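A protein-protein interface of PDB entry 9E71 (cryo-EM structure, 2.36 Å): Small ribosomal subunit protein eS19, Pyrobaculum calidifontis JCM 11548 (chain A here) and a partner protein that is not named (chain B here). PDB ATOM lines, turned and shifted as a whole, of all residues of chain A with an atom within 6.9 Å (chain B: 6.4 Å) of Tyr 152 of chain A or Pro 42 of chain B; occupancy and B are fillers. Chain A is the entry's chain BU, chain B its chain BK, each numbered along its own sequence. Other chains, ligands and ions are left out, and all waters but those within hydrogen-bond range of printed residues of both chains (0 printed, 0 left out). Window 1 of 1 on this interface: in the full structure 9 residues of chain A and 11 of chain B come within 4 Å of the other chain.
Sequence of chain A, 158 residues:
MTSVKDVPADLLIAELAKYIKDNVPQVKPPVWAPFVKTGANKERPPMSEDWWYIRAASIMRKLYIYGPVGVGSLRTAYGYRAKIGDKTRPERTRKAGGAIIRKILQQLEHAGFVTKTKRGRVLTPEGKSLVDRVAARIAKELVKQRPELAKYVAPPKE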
ATOM      1  N   THR A   2     -32.852 -20.542 -11.870  1.00  0.00           N
ATOM      2  CA  THR A   2     -32.450 -21.708 -12.644  1.00  0.00           C
ATOM      3  C   THR A   2     -31.037 -22.150 -12.291  1.00  0.00           C
ATOM      4  O   THR A   2     -30.669 -23.305 -12.496  1.00  0.00           O
ATOM      5  CB  THR A   2     -32.524 -21.434 -14.155  1.00  0.00           C
ATOM      6  OG1 THR A   2     -32.326 -22.659 -14.873  1.00  0.00           O
ATOM      7  CG2 THR A   2     -31.463 -20.425 -14.572  1.00  0.00           C
ATOM      8  N   SER A   3     -30.244 -21.226 -11.761  1.00  0.00           N
ATOM      9  CA  SER A   3     -28.884 -21.526 -11.350  1.00  0.00           C
ATOM     10  C   SER A   3     -28.630 -20.889  -9.995  1.00  0.00           C
ATOM     11  O   SER A   3     -29.385 -20.027  -9.542  1.00  0.00           O
ATOM     12  CB  SER A   3     -27.855 -21.039 -12.378  1.00  0.00           C
ATOM     13  OG  SER A   3     -27.657 -19.642 -12.291  1.00  0.00           O
ATOM     14  N   LYS A   5     -26.246 -18.911  -9.085  1.00  0.00           N
ATOM     15  CA  LYS A   5     -25.841 -17.519  -9.184  1.00  0.00           C
ATOM     16  C   LYS A   5     -26.981 -16.591  -9.588  1.00  0.00           C
ATOM     17  O   LYS A   5     -26.795 -15.372  -9.583  1.00  0.00           O
ATOM     18  CB  LYS A   5     -24.681 -17.384 -10.173  1.00  0.00           C
ATOM     19  CG  LYS A   5     -23.417 -18.099  -9.727  1.00  0.00           C
ATOM     20  CD  LYS A   5     -22.219 -17.699 -10.571  1.00  0.00           C
ATOM     21  CE  LYS A   5     -20.942 -18.363 -10.070  1.00  0.00           C
ATOM     22  NZ  LYS A   5     -19.733 -17.864 -10.779  1.00  0.00           N
ATOM     23  N   ASP A   6     -28.149 -17.131  -9.925  1.00  0.00           N
ATOM     24  CA  ASP A   6     -29.289 -16.326 -10.340  1.00  0.00           C
ATOM     25  C   ASP A   6     -30.255 -16.004  -9.205  1.00  0.00           C
ATOM     26  O   ASP A   6     -31.284 -15.371  -9.456  1.00  0.00           O
ATOM     27  CB  ASP A   6     -30.050 -17.030 -11.469  1.00  0.00           C
ATOM     28  CG  ASP A   6     -29.376 -16.873 -12.817  1.00  0.00           C
ATOM     29  OD1 ASP A   6     -28.179 -16.524 -12.852  1.00  0.00           O
ATOM     30  OD2 ASP A   6     -30.051 -17.084 -13.845  1.00  0.00           O
ATOM     31  N   VAL A   7     -29.958 -16.408  -7.973  1.00  0.00           N
ATOM     32  CA  VAL A   7     -30.825 -16.097  -6.837  1.00  0.00           C
ATOM     33  C   VAL A   7     -29.990 -15.510  -5.706  1.00  0.00           C
ATOM     34  O   VAL A   7     -28.794 -15.813  -5.600  1.00  0.00           O
ATOM     35  CB  VAL A   7     -31.591 -17.338  -6.357  1.00  0.00           C
ATOM     36  CG1 VAL A   7     -32.357 -17.968  -7.502  1.00  0.00           C
ATOM     37  CG2 VAL A   7     -30.641 -18.331  -5.727  1.00  0.00           C
ATOM     38  N   GLU A 148     -37.094  -7.235 -13.428  1.00  0.00           N
ATOM     39  CA  GLU A 148     -35.847  -7.100 -14.171  1.00  0.00           C
ATOM     40  C   GLU A 148     -35.095  -8.421 -14.255  1.00  0.00           C
ATOM     41  O   GLU A 148     -34.312  -8.626 -15.188  1.00  0.00           O
ATOM     42  CB  GLU A 148     -34.919  -6.036 -13.557  1.00  0.00           C
ATOM     43  CG  GLU A 148     -35.517  -4.735 -12.951  1.00  0.00           C
ATOM     44  CD  GLU A 148     -36.232  -4.911 -11.616  1.00  0.00           C
ATOM     45  OE1 GLU A 148     -35.571  -5.303 -10.632  1.00  0.00           O
ATOM     46  OE2 GLU A 148     -37.457  -4.673 -11.562  1.00  0.00           O
ATOM     47  N   LEU A 149     -35.314  -9.326 -13.301  1.00  0.00           N
ATOM     48  CA  LEU A 149     -34.570 -10.578 -13.278  1.00  0.00           C
ATOM     49  C   LEU A 149     -35.154 -11.630 -14.208  1.00  0.00           C
ATOM     50  O   LEU A 149     -34.606 -12.734 -14.278  1.00  0.00           O
ATOM     51  CB  LEU A 149     -34.521 -11.139 -11.860  1.00  0.00           C
ATOM     52  CG  LEU A 149     -34.279 -10.175 -10.703  1.00  0.00           C
ATOM     53  CD1 LEU A 149     -34.012 -10.971  -9.448  1.00  0.00           C
ATOM     54  CD2 LEU A 149     -33.121  -9.238 -10.997  1.00  0.00           C
ATOM     55  N   ALA A 150     -36.251 -11.324 -14.905  1.00  0.00           N
ATOM     56  CA  ALA A 150     -36.857 -12.306 -15.796  1.00  0.00           C
ATOM     57  C   ALA A 150     -35.935 -12.642 -16.960  1.00  0.00           C
ATOM     58  O   ALA A 150     -35.934 -13.774 -17.454  1.00  0.00           O
ATOM     59  CB  ALA A 150     -38.200 -11.791 -16.306  1.00  0.00           C
ATOM     60  N   LYS A 151     -35.117 -11.681 -17.393  1.00  0.00           N
ATOM     61  CA  LYS A 151     -34.198 -11.926 -18.498  1.00  0.00           C
ATOM     62  C   LYS A 151     -33.098 -12.914 -18.134  1.00  0.00           C
ATOM     63  O   LYS A 151     -32.451 -13.459 -19.033  1.00  0.00           O
ATOM     64  CB  LYS A 151     -33.573 -10.614 -18.970  1.00  0.00           C
ATOM     65  CG  LYS A 151     -32.901  -9.816 -17.872  1.00  0.00           C
ATOM     66  CD  LYS A 151     -32.139  -8.631 -18.436  1.00  0.00           C
ATOM     67  CE  LYS A 151     -32.951  -7.347 -18.353  1.00  0.00           C
ATOM     68  NZ  LYS A 151     -33.740  -7.246 -17.097  1.00  0.00           N
ATOM     69  N   TYR A 152     -32.859 -13.150 -16.848  1.00  0.00           N
ATOM     70  CA  TYR A 152     -31.819 -14.074 -16.424  1.00  0.00           C
ATOM     71  C   TYR A 152     -32.326 -15.488 -16.185  1.00  0.00           C
ATOM     72  O   TYR A 152     -31.516 -16.419 -16.134  1.00  0.00           O
ATOM     73  CB  TYR A 152     -31.154 -13.559 -15.146  1.00  0.00           C
ATOM     74  CG  TYR A 152     -30.655 -12.139 -15.246  1.00  0.00           C
ATOM     75  CD1 TYR A 152     -29.407 -11.863 -15.779  1.00  0.00           C
ATOM     76  CD2 TYR A 152     -31.433 -11.075 -14.809  1.00  0.00           C
ATOM     77  CE1 TYR A 152     -28.945 -10.569 -15.872  1.00  0.00           C
ATOM     78  CE2 TYR A 152     -30.979  -9.778 -14.897  1.00  0.00           C
ATOM     79  CZ  TYR A 152     -29.735  -9.530 -15.429  1.00  0.00           C
ATOM     80  OH  TYR A 152     -29.273  -8.240 -15.521  1.00  0.00           O
ATOM     81  N   VAL A 153     -33.636 -15.674 -16.037  1.00  0.00           N
ATOM     82  CA  VAL A 153     -34.221 -16.964 -15.696  1.00  0.00           C
ATOM     83  C   VAL A 153     -35.117 -17.483 -16.814  1.00  0.00           C
ATOM     84  O   VAL A 153     -34.982 -18.630 -17.253  1.00  0.00           O
ATOM     85  CB  VAL A 153     -34.998 -16.893 -14.364  1.00  0.00           C
ATOM     86  CG1 VAL A 153     -34.057 -17.122 -13.200  1.00  0.00           C
ATOM     87  CG2 VAL A 153     -35.706 -15.557 -14.231  1.00  0.00           C
ATOM     88  N   ALA A 154     -36.045 -16.651 -17.288  1.00  0.00           N
ATOM     89  CA  ALA A 154     -36.989 -17.011 -18.340  1.00  0.00           C
ATOM     90  C   ALA A 154     -36.896 -15.959 -19.437  1.00  0.00           C
ATOM     91  O   ALA A 154     -37.735 -15.048 -19.507  1.00  0.00           O
ATOM     92  CB  ALA A 154     -38.411 -17.117 -17.796  1.00  0.00           C
ATOM     93  N   PRO A 155     -35.877 -16.035 -20.288  1.00  0.00           N
ATOM     94  CA  PRO A 155     -35.728 -15.065 -21.378  1.00  0.00           C
ATOM     95  C   PRO A 155     -36.886 -15.151 -22.353  1.00  0.00           C
ATOM     96  O   PRO A 155     -37.406 -16.244 -22.619  1.00  0.00           O
ATOM     97  CB  PRO A 155     -34.412 -15.487 -22.046  1.00  0.00           C
ATOM     98  CG  PRO A 155     -33.674 -16.225 -20.991  1.00  0.00           C
ATOM     99  CD  PRO A 155     -34.716 -16.934 -20.186  1.00  0.00           C
ATOM    100  N   GLY B  34     -31.087  -7.336 -22.879  1.00  0.00           N
ATOM    101  CA  GLY B  34     -30.554  -6.338 -21.969  1.00  0.00           C
ATOM    102  C   GLY B  34     -29.851  -6.898 -20.747  1.00  0.00           C
ATOM    103  O   GLY B  34     -29.741  -6.211 -19.728  1.00  0.00           O
ATOM    104  N   ARG B  35     -29.372  -8.139 -20.825  1.00  0.00           N
ATOM    105  CA  ARG B  35     -28.691  -8.752 -19.697  1.00  0.00           C
ATOM    106  C   ARG B  35     -27.270  -8.215 -19.556  1.00  0.00           C
ATOM    107  O   ARG B  35     -26.696  -7.634 -20.480  1.00  0.00           O
ATOM    108  CB  ARG B  35     -28.651 -10.274 -19.832  1.00  0.00           C
ATOM    109  CG  ARG B  35     -29.899 -10.908 -20.405  1.00  0.00           C
ATOM    110  CD  ARG B  35     -29.670 -12.386 -20.670  1.00  0.00           C
ATOM    111  NE  ARG B  35     -29.327 -12.648 -22.062  1.00  0.00           N
ATOM    112  CZ  ARG B  35     -30.213 -12.847 -23.027  1.00  0.00           C
ATOM    113  NH1 ARG B  35     -31.512 -12.867 -22.779  1.00  0.00           N
ATOM    114  NH2 ARG B  35     -29.785 -13.039 -24.271  1.00  0.00           N
ATOM    115  N   VAL B  36     -26.709  -8.417 -18.369  1.00  0.00           N
ATOM    116  CA  VAL B  36     -25.323  -8.071 -18.072  1.00  0.00           C
ATOM    117  C   VAL B  36     -24.894  -8.869 -16.850  1.00  0.00           C
ATOM    118  O   VAL B  36     -25.603  -8.897 -15.840  1.00  0.00           O
ATOM    119  CB  VAL B  36     -25.149  -6.556 -17.847  1.00  0.00           C
ATOM    120  CG1 VAL B  36     -26.250  -6.023 -16.955  1.00  0.00           C
ATOM    121  CG2 VAL B  36     -23.794  -6.266 -17.246  1.00  0.00           C
ATOM    122  N   ARG B  37     -23.733  -9.513 -16.936  1.00  0.00           N
ATOM    123  CA  ARG B  37     -23.283 -10.456 -15.917  1.00  0.00           C
ATOM    124  C   ARG B  37     -21.823 -10.207 -15.586  1.00  0.00           C
ATOM    125  O   ARG B  37     -20.962 -10.282 -16.468  1.00  0.00           O
ATOM    126  CB  ARG B  37     -23.462 -11.900 -16.383  1.00  0.00           C
ATOM    127  CG  ARG B  37     -24.885 -12.373 -16.368  1.00  0.00           C
ATOM    128  CD  ARG B  37     -24.965 -13.779 -15.832  1.00  0.00           C
ATOM    129  NE  ARG B  37     -26.003 -14.550 -16.497  1.00  0.00           N
ATOM    130  CZ  ARG B  37     -26.750 -15.463 -15.894  1.00  0.00           C
ATOM    131  NH1 ARG B  37     -26.586 -15.755 -14.615  1.00  0.00           N
ATOM    132  NH2 ARG B  37     -27.692 -16.091 -16.589  1.00  0.00           N
ATOM    133  N   ILE B  38     -21.546  -9.928 -14.318  1.00  0.00           N
ATOM    134  CA  ILE B  38     -20.181  -9.840 -13.823  1.00  0.00           C
ATOM    135  C   ILE B  38     -19.854 -11.128 -13.083  1.00  0.00           C
ATOM    136  O   ILE B  38     -20.482 -11.446 -12.068  1.00  0.00           O
ATOM    137  CB  ILE B  38     -19.991  -8.618 -12.914  1.00  0.00           C
ATOM    138  CG1 ILE B  38     -20.138  -7.328 -13.723  1.00  0.00           C
ATOM    139  CG2 ILE B  38     -18.632  -8.671 -12.249  1.00  0.00           C
ATOM    140  CD1 ILE B  38     -21.522  -6.756 -13.719  1.00  0.00           C
ATOM    141  N   GLY B  40     -20.401 -14.157 -13.747  1.00  0.00           N
ATOM    142  CA  GLY B  40     -21.482 -15.114 -13.727  1.00  0.00           C
ATOM    143  C   GLY B  40     -22.660 -14.735 -12.858  1.00  0.00           C
ATOM    144  O   GLY B  40     -23.606 -15.524 -12.751  1.00  0.00           O
ATOM    145  N   TYR B  41     -22.632 -13.563 -12.228  1.00  0.00           N
ATOM    146  CA  TYR B  41     -23.738 -13.097 -11.406  1.00  0.00           C
ATOM    147  C   TYR B  41     -24.489 -11.980 -12.110  1.00  0.00           C
ATOM    148  O   TYR B  41     -23.869 -11.111 -12.727  1.00  0.00           O
ATOM    149  CB  TYR B  41     -23.244 -12.583 -10.052  1.00  0.00           C
ATOM    150  CG  TYR B  41     -22.479 -13.596  -9.237  1.00  0.00           C
ATOM    151  CD1 TYR B  41     -21.115 -13.769  -9.410  1.00  0.00           C
ATOM    152  CD2 TYR B  41     -23.122 -14.381  -8.294  1.00  0.00           C
ATOM    153  CE1 TYR B  41     -20.414 -14.696  -8.673  1.00  0.00           C
ATOM    154  CE2 TYR B  41     -22.429 -15.311  -7.548  1.00  0.00           C
ATOM    155  CZ  TYR B  41     -21.074 -15.465  -7.743  1.00  0.00           C
ATOM    156  OH  TYR B  41     -20.367 -16.387  -7.008  1.00  0.00           O
ATOM    157  N   PRO B  42     -25.817 -11.990 -12.047  1.00  0.00           N
ATOM    158  CA  PRO B  42     -26.588 -10.891 -12.635  1.00  0.00           C
ATOM    159  C   PRO B  42     -26.315  -9.570 -11.927  1.00  0.00           C
ATOM    160  O   PRO B  42     -25.952  -9.536 -10.750  1.00  0.00           O
ATOM    161  CB  PRO B  42     -28.042 -11.343 -12.456  1.00  0.00           C
ATOM    162  CG  PRO B  42     -27.961 -12.822 -12.304  1.00  0.00           C
ATOM    163  CD  PRO B  42     -26.676 -13.095 -11.598  1.00  0.00           C
ATOM    164  N   LEU B  43     -26.474  -8.476 -12.675  1.00  0.00           N
ATOM    165  CA  LEU B  43     -26.178  -7.151 -12.139  1.00  0.00           C
ATOM    166  C   LEU B  43     -27.131  -6.767 -11.020  1.00  0.00           C
ATOM    167  O   LEU B  43     -26.739  -6.066 -10.083  1.00  0.00           O
ATOM    168  CB  LEU B  43     -26.232  -6.108 -13.252  1.00  0.00           C
ATOM    169  CG  LEU B  43     -24.936  -5.350 -13.519  1.00  0.00           C
ATOM    170  CD1 LEU B  43     -25.200  -4.149 -14.401  1.00  0.00           C
ATOM    171  CD2 LEU B  43     -24.335  -4.907 -12.207  1.00  0.00           C
ATOM    172  N   GLU B  44     -28.383  -7.206 -11.094  1.00  0.00           N
ATOM    173  CA  GLU B  44     -29.393  -6.751 -10.142  1.00  0.00           C
ATOM    174  C   GLU B  44     -29.539  -7.770  -9.018  1.00  0.00           C
ATOM    175  O   GLU B  44     -30.578  -7.883  -8.370  1.00  0.00           O
ATOM    176  CB  GLU B  44     -30.724  -6.497 -10.844  1.00  0.00           C
ATOM    177  CG  GLU B  44     -30.689  -5.374 -11.870  1.00  0.00           C
ATOM    178  CD  GLU B  44     -30.236  -5.839 -13.236  1.00  0.00           C
ATOM    179  OE1 GLU B  44     -29.230  -6.569 -13.297  1.00  0.00           O
ATOM    180  OE2 GLU B  44     -30.871  -5.469 -14.242  1.00  0.00           O
ATOM    181  N   LEU B  45     -28.459  -8.504  -8.767  1.00  0.00           N
ATOM    182  CA  LEU B  45     -28.359  -9.366  -7.598  1.00  0.00           C
ATOM    183  C   LEU B  45     -27.037  -9.109  -6.895  1.00  0.00           C
ATOM    184  O   LEU B  45     -26.652  -9.851  -5.985  1.00  0.00           O
ATOM    185  CB  LEU B  45     -28.470 -10.844  -7.975  1.00  0.00           C
ATOM    186  CG  LEU B  45     -29.737 -11.437  -8.583  1.00  0.00           C
ATOM    187  CD1 LEU B  45     -29.752 -12.901  -8.266  1.00  0.00           C
ATOM    188  CD2 LEU B  45     -30.967 -10.807  -8.003  1.00  0.00           C
ATOM    189  N   TRP B  46     -26.333  -8.076  -7.321  1.00  0.00           N
ATOM    190  CA  TRP B  46     -25.039  -7.762  -6.738  1.00  0.00           C
ATOM    191  C   TRP B  46     -25.233  -7.264  -5.312  1.00  0.00           C
ATOM    192  O   TRP B  46     -25.967  -6.293  -5.100  1.00  0.00           O
ATOM    193  CB  TRP B  46     -24.324  -6.722  -7.580  1.00  0.00           C
ATOM    194  CG  TRP B  46     -22.876  -6.649  -7.298  1.00  0.00           C
ATOM    195  CD1 TRP B  46     -22.224  -5.672  -6.615  1.00  0.00           C
ATOM    196  CD2 TRP B  46     -21.884  -7.597  -7.691  1.00  0.00           C
ATOM    197  NE1 TRP B  46     -20.885  -5.950  -6.556  1.00  0.00           N
ATOM    198  CE2 TRP B  46     -20.650  -7.129  -7.214  1.00  0.00           C
ATOM    199  CE3 TRP B  46     -21.919  -8.797  -8.404  1.00  0.00           C
ATOM    200  CZ2 TRP B  46     -19.462  -7.818  -7.424  1.00  0.00           C
ATOM    201  CZ3 TRP B  46     -20.740  -9.477  -8.613  1.00  0.00           C
ATOM    202  CH2 TRP B  46     -19.528  -8.988  -8.123  1.00  0.00           C
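The side-chain carboxylate of Asp 6 of chain A lies within salt-bridge range of the guanidinium group of Arg 37 of chain B (2.5 Å). The side-chain hydroxyl (OH) of Tyr 152 of chain A is in hydrogen-bond range of the side-chain carboxylate (OE1) of Glu 44 of chain B, at 2.8 Å.
Of the printed residues of chain B, Lys 5 of chain A touches Gly 40, Tyr 41 and Pro 42. Of the printed residues of chain B, Tyr 152 of chain A touches Arg 35 (3.98 Å), Val 36 (3.7 Å), Arg 37 (3.9 Å), Pro 42 (3.6 Å), Leu 43 (3.999 Å) and Glu 44 (2.8 Å). Val 153 of chain A touches none of the printed residues of chain B. Printed residues of chain A within 4 Å of Arg 37 of chain B: Asp 6 and Tyr 152. Of chain A, only Lys 5, Asp 6 and Tyr 152 come within 4 Å of Pro 42 of chain B. Printed residues of chain A within 4 Å of Glu 44 of chain B: Leu 149 (3.6 Å) and Tyr 152 (2.8 Å). The nearest residue of chain A that does not touch Pro 42 of chain B is Leu 149 of chain A (5.7 Å).
Along chain B the printed residues that touch a printed residue of chain A span positions 34 to 45. Among the printed residues, 18 pairs touch across the chains.
Among the printed residues, pairs that only touch across the chains: Lys 5 of chain A with Pro 42 of chain B, Asp 6 of chain A with Leu 45 of chain B, Lys 5 of chain A with Gly 40 of chain B, Leu 149 of chain A with Leu 45 of chain B, Lys 151 of chain A with Arg 35 of chain B, Val 7 of chain A with Leu 45 of chain B, Tyr 152 of chain A with Pro 42 of chain B, Lys 151 of chain A with Gly 34 of chain B, Leu 149 of chain A with Glu 44 of chain B, Lys 5 of chain A with Tyr 41 of chain B, Tyr 152 of chain A with Val 36 of chain B, Asp 6 of chain A with Pro 42 of chain B, Tyr 152 of chain A with Arg 37 of chain B, Pro 155 of chain A with Arg 35 of chain B, Tyr 152 of chain A with Arg 35 of chain B and Tyr 152 of chain A with Leu 43 of chain B.
The side-chain hydroxyl (OG) of Ser 3 of chain A sits at hydrogen-bond distance from the side-chain carboxylate (OD1) of Asp 6 of chain A (3.2 Å). O of Glu 148 of chain A lies within hydrogen-bond range of NZ of Lys 151 of chain A, at 2.4 Å. O of Val 36 of chain B sits at hydrogen-bond distance from N of Leu 43 of chain B (3.3 Å).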
